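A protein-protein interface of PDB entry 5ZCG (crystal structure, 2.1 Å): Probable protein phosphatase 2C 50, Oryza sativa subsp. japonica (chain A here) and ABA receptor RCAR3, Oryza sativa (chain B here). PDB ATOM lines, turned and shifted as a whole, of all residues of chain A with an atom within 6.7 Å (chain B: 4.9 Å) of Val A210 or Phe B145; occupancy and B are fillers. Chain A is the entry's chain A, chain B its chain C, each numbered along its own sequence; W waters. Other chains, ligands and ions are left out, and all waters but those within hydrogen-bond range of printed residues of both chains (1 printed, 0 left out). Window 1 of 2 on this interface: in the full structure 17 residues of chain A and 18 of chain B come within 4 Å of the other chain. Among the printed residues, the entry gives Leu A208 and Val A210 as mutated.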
ATOM      1  N   LYS A 198      23.430  13.817   3.950  1.00  0.00           N
ATOM      2  CA  LYS A 198      22.656  14.440   5.009  1.00  0.00           C
ATOM      3  C   LYS A 198      22.133  13.384   5.968  1.00  0.00           C
ATOM      4  O   LYS A 198      21.729  12.294   5.552  1.00  0.00           O
ATOM      5  CB  LYS A 198      21.474  15.235   4.442  1.00  0.00           C
ATOM      6  CG  LYS A 198      21.794  16.663   4.038  1.00  0.00           C
ATOM      7  CD  LYS A 198      20.516  17.486   3.911  1.00  0.00           C
ATOM      8  CE  LYS A 198      20.779  18.963   4.159  1.00  0.00           C
ATOM      9  NZ  LYS A 198      19.561  19.677   4.638  1.00  0.00           N
ATOM     10  N   ILE A 200      19.123  13.314   8.573  1.00  0.00           N
ATOM     11  CA  ILE A 200      17.917  14.096   8.818  1.00  0.00           C
ATOM     12  C   ILE A 200      17.035  13.337   9.798  1.00  0.00           C
ATOM     13  O   ILE A 200      16.792  12.141   9.621  1.00  0.00           O
ATOM     14  CB  ILE A 200      17.153  14.392   7.512  1.00  0.00           C
ATOM     15  CG1 ILE A 200      18.057  15.133   6.527  1.00  0.00           C
ATOM     16  CG2 ILE A 200      15.899  15.209   7.802  1.00  0.00           C
ATOM     17  CD1 ILE A 200      17.707  14.901   5.074  1.00  0.00           C
ATOM     18  N   TRP A 202      13.856  12.244  10.638  1.00  0.00           N
ATOM     19  CA  TRP A 202      12.573  12.059   9.954  1.00  0.00           C
ATOM     20  C   TRP A 202      12.026  10.714  10.425  1.00  0.00           C
ATOM     21  O   TRP A 202      12.291   9.683   9.800  1.00  0.00           O
ATOM     22  CB  TRP A 202      12.760  12.103   8.444  1.00  0.00           C
ATOM     23  CG  TRP A 202      11.520  12.377   7.667  1.00  0.00           C
ATOM     24  CD1 TRP A 202      10.512  11.496   7.385  1.00  0.00           C
ATOM     25  CD2 TRP A 202      11.154  13.618   7.048  1.00  0.00           C
ATOM     26  NE1 TRP A 202       9.543  12.115   6.630  1.00  0.00           N
ATOM     27  CE2 TRP A 202       9.913  13.417   6.412  1.00  0.00           C
ATOM     28  CE3 TRP A 202      11.760  14.879   6.968  1.00  0.00           C
ATOM     29  CZ2 TRP A 202       9.262  14.432   5.708  1.00  0.00           C
ATOM     30  CZ3 TRP A 202      11.111  15.886   6.269  1.00  0.00           C
ATOM     31  CH2 TRP A 202       9.877  15.655   5.645  1.00  0.00           C
ATOM     32  N   ARG A 206      17.915   9.536  10.071  1.00  0.00           N
ATOM     33  CA  ARG A 206      18.044   8.674   8.909  1.00  0.00           C
ATOM     34  C   ARG A 206      19.017   9.267   7.899  1.00  0.00           C
ATOM     35  O   ARG A 206      19.133  10.494   7.764  1.00  0.00           O
ATOM     36  CB  ARG A 206      16.684   8.440   8.241  1.00  0.00           C
ATOM     37  CG  ARG A 206      15.660   7.785   9.161  1.00  0.00           C
ATOM     38  CD  ARG A 206      14.276   7.752   8.544  1.00  0.00           C
ATOM     39  NE  ARG A 206      13.317   7.053   9.398  1.00  0.00           N
ATOM     40  CZ  ARG A 206      13.129   5.735   9.373  1.00  0.00           C
ATOM     41  NH1 ARG A 206      13.834   4.979   8.540  1.00  0.00           N
ATOM     42  NH2 ARG A 206      12.244   5.169  10.181  1.00  0.00           N
ATOM     43  N   VAL A 207      19.712   8.372   7.191  1.00  0.00           N
ATOM     44  CA  VAL A 207      20.610   8.746   6.101  1.00  0.00           C
ATOM     45  C   VAL A 207      19.782   9.284   4.943  1.00  0.00           C
ATOM     46  O   VAL A 207      18.959   8.562   4.368  1.00  0.00           O
ATOM     47  CB  VAL A 207      21.457   7.549   5.650  1.00  0.00           C
ATOM     48  CG1 VAL A 207      22.405   7.972   4.543  1.00  0.00           C
ATOM     49  CG2 VAL A 207      22.221   6.950   6.823  1.00  0.00           C
ATOM     50  N   LEU A 208      20.021  10.545   4.579  1.00  0.00           N
ATOM     51  CA  LEU A 208      19.214  11.297   3.622  1.00  0.00           C
ATOM     52  C   LEU A 208      17.753  11.394   4.050  1.00  0.00           C
ATOM     53  O   LEU A 208      16.894  11.763   3.241  1.00  0.00           O
ATOM     54  CB  LEU A 208      19.304  10.705   2.205  1.00  0.00           C
ATOM     55  CG  LEU A 208      20.686  10.296   1.673  1.00  0.00           C
ATOM     56  CD1 LEU A 208      20.585   9.907   0.209  1.00  0.00           C
ATOM     57  CD2 LEU A 208      21.701  11.408   1.853  1.00  0.00           C
ATOM     58  N   GLY A 209      17.450  11.082   5.308  1.00  0.00           N
ATOM     59  CA  GLY A 209      16.081  11.034   5.778  1.00  0.00           C
ATOM     60  C   GLY A 209      15.353   9.746   5.470  1.00  0.00           C
ATOM     61  O   GLY A 209      14.162   9.648   5.775  1.00  0.00           O
ATOM     62  N   VAL A 210      16.025   8.757   4.878  1.00  0.00           N
ATOM     63  CA  VAL A 210      15.376   7.552   4.365  1.00  0.00           C
ATOM     64  C   VAL A 210      15.626   6.339   5.268  1.00  0.00           C
ATOM     65  O   VAL A 210      14.682   5.716   5.758  1.00  0.00           O
ATOM     66  CB  VAL A 210      15.815   7.266   2.912  1.00  0.00           C
ATOM     67  CG1 VAL A 210      15.230   5.943   2.429  1.00  0.00           C
ATOM     68  CG2 VAL A 210      15.403   8.406   1.995  1.00  0.00           C
ATOM     69  N   LEU A 211      16.889   6.015   5.527  1.00  0.00           N
ATOM     70  CA  LEU A 211      17.270   4.753   6.147  1.00  0.00           C
ATOM     71  C   LEU A 211      17.804   5.010   7.546  1.00  0.00           C
ATOM     72  O   LEU A 211      18.693   5.846   7.733  1.00  0.00           O
ATOM     73  CB  LEU A 211      18.331   4.036   5.300  1.00  0.00           C
ATOM     74  CG  LEU A 211      18.670   2.579   5.618  1.00  0.00           C
ATOM     75  CD1 LEU A 211      17.565   1.664   5.115  1.00  0.00           C
ATOM     76  CD2 LEU A 211      19.994   2.197   4.994  1.00  0.00           C
ATOM     77  N   ALA A 212      17.264   4.283   8.524  1.00  0.00           N
ATOM     78  CA  ALA A 212      17.572   4.503   9.930  1.00  0.00           C
ATOM     79  C   ALA A 212      18.831   3.777  10.380  1.00  0.00           C
ATOM     80  O   ALA A 212      18.987   3.511  11.576  1.00  0.00           O
ATOM     81  CB  ALA A 212      16.380   4.091  10.803  1.00  0.00           C
ATOM     82  N   MET A 213      19.722   3.450   9.450  1.00  0.00           N
ATOM     83  CA  MET A 213      21.004   2.844   9.757  1.00  0.00           C
ATOM     84  C   MET A 213      22.048   3.391   8.794  1.00  0.00           C
ATOM     85  O   MET A 213      21.747   3.707   7.639  1.00  0.00           O
ATOM     86  CB  MET A 213      20.961   1.318   9.645  1.00  0.00           C
ATOM     87  CG  MET A 213      20.695   0.807   8.238  1.00  0.00           C
ATOM     88  SD  MET A 213      20.629  -0.991   8.206  1.00  0.00           S
ATOM     89  CE  MET A 213      20.151  -1.272   9.878  1.00  0.00           C
ATOM     90  N   TYR A 221      21.592   1.829  -3.634  1.00  0.00           N
ATOM     91  CA  TYR A 221      21.128   3.163  -3.995  1.00  0.00           C
ATOM     92  C   TYR A 221      21.530   4.217  -2.975  1.00  0.00           C
ATOM     93  O   TYR A 221      21.436   5.410  -3.280  1.00  0.00           O
ATOM     94  CB  TYR A 221      19.608   3.175  -4.182  1.00  0.00           C
ATOM     95  CG  TYR A 221      18.805   3.206  -2.896  1.00  0.00           C
ATOM     96  CD1 TYR A 221      18.935   2.202  -1.942  1.00  0.00           C
ATOM     97  CD2 TYR A 221      17.897   4.227  -2.646  1.00  0.00           C
ATOM     98  CE1 TYR A 221      18.193   2.224  -0.774  1.00  0.00           C
ATOM     99  CE2 TYR A 221      17.151   4.256  -1.480  1.00  0.00           C
ATOM    100  CZ  TYR A 221      17.301   3.251  -0.551  1.00  0.00           C
ATOM    101  OH  TYR A 221      16.565   3.273   0.610  1.00  0.00           O
ATOM    102  N   LEU A 222      22.001   3.810  -1.797  1.00  0.00           N
ATOM    103  CA  LEU A 222      22.417   4.741  -0.756  1.00  0.00           C
ATOM    104  C   LEU A 222      23.929   4.802  -0.596  1.00  0.00           C
ATOM    105  O   LEU A 222      24.418   5.391   0.378  1.00  0.00           O
ATOM    106  CB  LEU A 222      21.750   4.379   0.573  1.00  0.00           C
ATOM    107  CG  LEU A 222      20.283   4.807   0.645  1.00  0.00           C
ATOM    108  CD1 LEU A 222      19.628   4.350   1.936  1.00  0.00           C
ATOM    109  CD2 LEU A 222      20.171   6.314   0.497  1.00  0.00           C
ATOM    110  N   GLY B  72      11.831  -0.505   6.042  1.00  0.00           N
ATOM    111  CA  GLY B  72      13.021   0.320   6.125  1.00  0.00           C
ATOM    112  C   GLY B  72      12.801   1.811   5.944  1.00  0.00           C
ATOM    113  O   GLY B  72      13.725   2.592   6.210  1.00  0.00           O
ATOM    114  N   LEU B  73      11.603   2.237   5.516  1.00  0.00           N
ATOM    115  CA  LEU B  73      11.262   3.619   5.201  1.00  0.00           C
ATOM    116  C   LEU B  73      10.680   4.339   6.415  1.00  0.00           C
ATOM    117  O   LEU B  73      10.287   3.705   7.397  1.00  0.00           O
ATOM    118  CB  LEU B  73      10.262   3.648   4.044  1.00  0.00           C
ATOM    119  CG  LEU B  73      10.820   3.241   2.680  1.00  0.00           C
ATOM    120  CD1 LEU B  73       9.707   3.134   1.653  1.00  0.00           C
ATOM    121  CD2 LEU B  73      11.879   4.229   2.225  1.00  0.00           C
ATOM    122  N   PRO B  74      10.622   5.677   6.386  1.00  0.00           N
ATOM    123  CA  PRO B  74      10.024   6.413   7.514  1.00  0.00           C
ATOM    124  C   PRO B  74       8.533   6.180   7.687  1.00  0.00           C
ATOM    125  O   PRO B  74       7.993   6.546   8.737  1.00  0.00           O
ATOM    126  CB  PRO B  74      10.309   7.883   7.168  1.00  0.00           C
ATOM    127  CG  PRO B  74      11.418   7.849   6.192  1.00  0.00           C
ATOM    128  CD  PRO B  74      11.241   6.591   5.411  1.00  0.00           C
ATOM    129  N   LEU B 103       4.375  13.824   5.177  1.00  0.00           N
ATOM    130  CA  LEU B 103       4.309  14.681   3.997  1.00  0.00           C
ATOM    131  C   LEU B 103       2.876  15.175   3.830  1.00  0.00           C
ATOM    132  O   LEU B 103       2.139  14.754   2.931  1.00  0.00           O
ATOM    133  CB  LEU B 103       4.799  13.922   2.760  1.00  0.00           C
ATOM    134  CG  LEU B 103       6.261  13.464   2.773  1.00  0.00           C
ATOM    135  CD1 LEU B 103       6.574  12.663   1.524  1.00  0.00           C
ATOM    136  CD2 LEU B 103       7.204  14.655   2.885  1.00  0.00           C
ATOM    137  N   GLU B 141      15.760  20.357   4.445  1.00  0.00           N
ATOM    138  CA  GLU B 141      15.728  18.924   4.725  1.00  0.00           C
ATOM    139  C   GLU B 141      14.565  18.250   4.008  1.00  0.00           C
ATOM    140  O   GLU B 141      14.717  17.152   3.458  1.00  0.00           O
ATOM    141  CB  GLU B 141      15.617  18.685   6.230  1.00  0.00           C
ATOM    142  CG  GLU B 141      16.834  19.085   7.040  1.00  0.00           C
ATOM    143  CD  GLU B 141      16.588  18.955   8.531  1.00  0.00           C
ATOM    144  OE1 GLU B 141      15.463  19.265   8.980  1.00  0.00           O
ATOM    145  OE2 GLU B 141      17.515  18.530   9.251  1.00  0.00           O
ATOM    146  N   THR B 142      13.389  18.893   4.017  1.00  0.00           N
ATOM    147  CA  THR B 142      12.205  18.307   3.394  1.00  0.00           C
ATOM    148  C   THR B 142      12.396  18.160   1.890  1.00  0.00           C
ATOM    149  O   THR B 142      12.095  17.106   1.308  1.00  0.00           O
ATOM    150  CB  THR B 142      10.977  19.167   3.707  1.00  0.00           C
ATOM    151  OG1 THR B 142      10.881  19.370   5.124  1.00  0.00           O
ATOM    152  CG2 THR B 142       9.703  18.494   3.212  1.00  0.00           C
ATOM    153  N   CYS B 143      12.913  19.208   1.243  1.00  0.00           N
ATOM    154  CA  CYS B 143      13.207  19.112  -0.182  1.00  0.00           C
ATOM    155  C   CYS B 143      14.268  18.049  -0.461  1.00  0.00           C
ATOM    156  O   CYS B 143      14.156  17.296  -1.432  1.00  0.00           O
ATOM    157  CB  CYS B 143      13.656  20.469  -0.721  1.00  0.00           C
ATOM    158  SG  CYS B 143      12.322  21.673  -0.827  1.00  0.00           S
ATOM    159  N   TYR B 144      15.299  17.963   0.383  1.00  0.00           N
ATOM    160  CA  TYR B 144      16.348  16.968   0.171  1.00  0.00           C
ATOM    161  C   TYR B 144      15.788  15.551   0.229  1.00  0.00           C
ATOM    162  O   TYR B 144      16.101  14.708  -0.626  1.00  0.00           O
ATOM    163  CB  TYR B 144      17.439  17.165   1.222  1.00  0.00           C
ATOM    164  CG  TYR B 144      18.708  16.388   0.984  1.00  0.00           C
ATOM    165  CD1 TYR B 144      19.745  16.929   0.234  1.00  0.00           C
ATOM    166  CD2 TYR B 144      18.882  15.122   1.526  1.00  0.00           C
ATOM    167  CE1 TYR B 144      20.915  16.228   0.021  1.00  0.00           C
ATOM    168  CE2 TYR B 144      20.051  14.410   1.319  1.00  0.00           C
ATOM    169  CZ  TYR B 144      21.066  14.969   0.566  1.00  0.00           C
ATOM    170  OH  TYR B 144      22.236  14.265   0.354  1.00  0.00           O
ATOM    171  N   PHE B 145      14.934  15.285   1.222  1.00  0.00           N
ATOM    172  CA  PHE B 145      14.327  13.966   1.392  1.00  0.00           C
ATOM    173  C   PHE B 145      13.424  13.612   0.208  1.00  0.00           C
ATOM    174  O   PHE B 145      13.544  12.528  -0.394  1.00  0.00           O
ATOM    175  CB  PHE B 145      13.558  13.965   2.720  1.00  0.00           C
ATOM    176  CG  PHE B 145      12.638  12.796   2.911  1.00  0.00           C
ATOM    177  CD1 PHE B 145      13.140  11.539   3.204  1.00  0.00           C
ATOM    178  CD2 PHE B 145      11.264  12.961   2.828  1.00  0.00           C
ATOM    179  CE1 PHE B 145      12.287  10.464   3.391  1.00  0.00           C
ATOM    180  CE2 PHE B 145      10.410  11.890   3.014  1.00  0.00           C
ATOM    181  CZ  PHE B 145      10.925  10.640   3.298  1.00  0.00           C
ATOM    182  N   VAL B 146      12.516  14.524  -0.150  1.00  0.00           N
ATOM    183  CA  VAL B 146      11.609  14.234  -1.256  1.00  0.00           C
ATOM    184  C   VAL B 146      12.394  14.054  -2.548  1.00  0.00           C
ATOM    185  O   VAL B 146      12.078  13.180  -3.366  1.00  0.00           O
ATOM    186  CB  VAL B 146      10.541  15.335  -1.388  1.00  0.00           C
ATOM    187  CG1 VAL B 146       9.656  15.055  -2.589  1.00  0.00           C
ATOM    188  CG2 VAL B 146       9.705  15.424  -0.121  1.00  0.00           C
ATOM    189  N   GLU B 147      13.433  14.873  -2.750  1.00  0.00           N
ATOM    190  CA  GLU B 147      14.250  14.763  -3.951  1.00  0.00           C
ATOM    191  C   GLU B 147      14.938  13.411  -4.025  1.00  0.00           C
ATOM    192  O   GLU B 147      14.983  12.797  -5.093  1.00  0.00           O
ATOM    193  CB  GLU B 147      15.292  15.881  -3.986  1.00  0.00           C
ATOM    194  CG  GLU B 147      14.757  17.237  -4.430  1.00  0.00           C
ATOM    195  CD  GLU B 147      15.712  18.369  -4.085  1.00  0.00           C
ATOM    196  OE1 GLU B 147      15.277  19.541  -4.062  1.00  0.00           O
ATOM    197  OE2 GLU B 147      16.904  18.081  -3.837  1.00  0.00           O
ATOM    198  N   ALA B 148      15.488  12.930  -2.907  1.00  0.00           N
ATOM    199  CA  ALA B 148      16.127  11.614  -2.931  1.00  0.00           C
ATOM    200  C   ALA B 148      15.142  10.541  -3.379  1.00  0.00           C
ATOM    201  O   ALA B 148      15.456   9.712  -4.253  1.00  0.00           O
ATOM    202  CB  ALA B 148      16.700  11.279  -1.554  1.00  0.00           C
ATOM    203  N   LEU B 149      13.919  10.576  -2.824  1.00  0.00           N
ATOM    204  CA  LEU B 149      12.923   9.570  -3.196  1.00  0.00           C
ATOM    205  C   LEU B 149      12.513   9.700  -4.663  1.00  0.00           C
ATOM    206  O   LEU B 149      12.458   8.702  -5.398  1.00  0.00           O
ATOM    207  CB  LEU B 149      11.698   9.686  -2.287  1.00  0.00           C
ATOM    208  CG  LEU B 149      11.944   9.362  -0.812  1.00  0.00           C
ATOM    209  CD1 LEU B 149      10.689   9.581   0.009  1.00  0.00           C
ATOM    210  CD2 LEU B 149      12.453   7.936  -0.653  1.00  0.00           C
HETATM  211  O   HOH W   1      15.468   2.151   8.010  1.00  0.00           O
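O of Gly B72 sits close to O of Val A210 (3.3 Å).
The guanidinium group (NH1) of Arg A206 lies within hydrogen-bond range of the backbone carbonyl oxygen (O) of Gly B72, at 3.3 Å.
The guanidinium group (NE) of Arg A206 is in hydrogen-bond range of the backbone carbonyl oxygen (O) of Trp A202, 2.9 Å away.
The backbone NH (N) of Arg A206 sits at hydrogen-bond distance from the backbone carbonyl oxygen (O) of Ile A200 (2.9 Å).
The backbone carbonyl oxygen (O) of Lys A198 sits at hydrogen-bond distance from the backbone NH (N) of Leu A208, at 2.6 Å.
The guanidinium group (NH1) of Arg A206 is in hydrogen-bond range of the backbone carbonyl oxygen (O) of Val A210.
Among the printed residues, pairs that only touch across the chains: Gly A209 with Phe B145, Leu A208 with Tyr B144, Gly A209 with Pro B74, Trp A202 with Leu B103, Lys A198 with Tyr B144, Val A210 with Pro B74, Trp A202 with Pro B74, Trp A202 with Thr B142, Arg A206 with Pro B74, Lys A198 with Glu B141, Arg A206 with Leu B73, Trp A202 with Phe B145, Ile A200 with Tyr B144, Leu A208 with Phe B145, Val A210 with Leu B73, Ile A200 with Glu B141, Val A210 with Phe B145 and Val A210 with Leu B149.
Printed residues of chain B within 4 Å of Val A210: Gly B72, Leu B73, Pro B74, Phe B145 and Leu B149.
Of the printed residues of chain A, Phe B145 touches Trp A202 (3.7 Å), Leu A208 (3.8 Å), Gly A209 (3.1 Å) and Val A210 (3.99 Å).
Printed residues of chain B within 4 Å of Ile A200: Glu B141 (3.8 Å) and Tyr B144 (3.7 Å).
Of the printed residues of chain B, Leu A208 touches Tyr B144 and Phe B145.
Ala B148 touches none of the printed residues of chain A.
Glu B147 touches none of the printed residues of chain A.
The nearest printed residue of chain B that does not touch Val A210 is Ala B148 (4.7 Å).
The nearest printed residue of chain A that does not touch Phe B145 is Ile A200 (4.8 Å).
Of the 13 printed residues of chain B, 9 touch a printed residue of chain A.
Hydrophobic or aromatic side chains of chain B that line the printed part of chain A: Leu B73, Pro B74, Leu B103, Tyr B144, Phe B145 and Leu B149.
Printed residues of chain A that touch a printed residue of chain B: Lys A198, Ile A200, Trp A202, Arg A206, Leu A208, Gly A209 and Val A210.
Among the printed residues, 20 pairs touch across the chains.
Water W1 lies within hydrogen-bond range of O of Gly B72 (2.5 Å), N of Ala A212 (2.8 Å) and NH1 of Arg A206 (3.3 Å).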
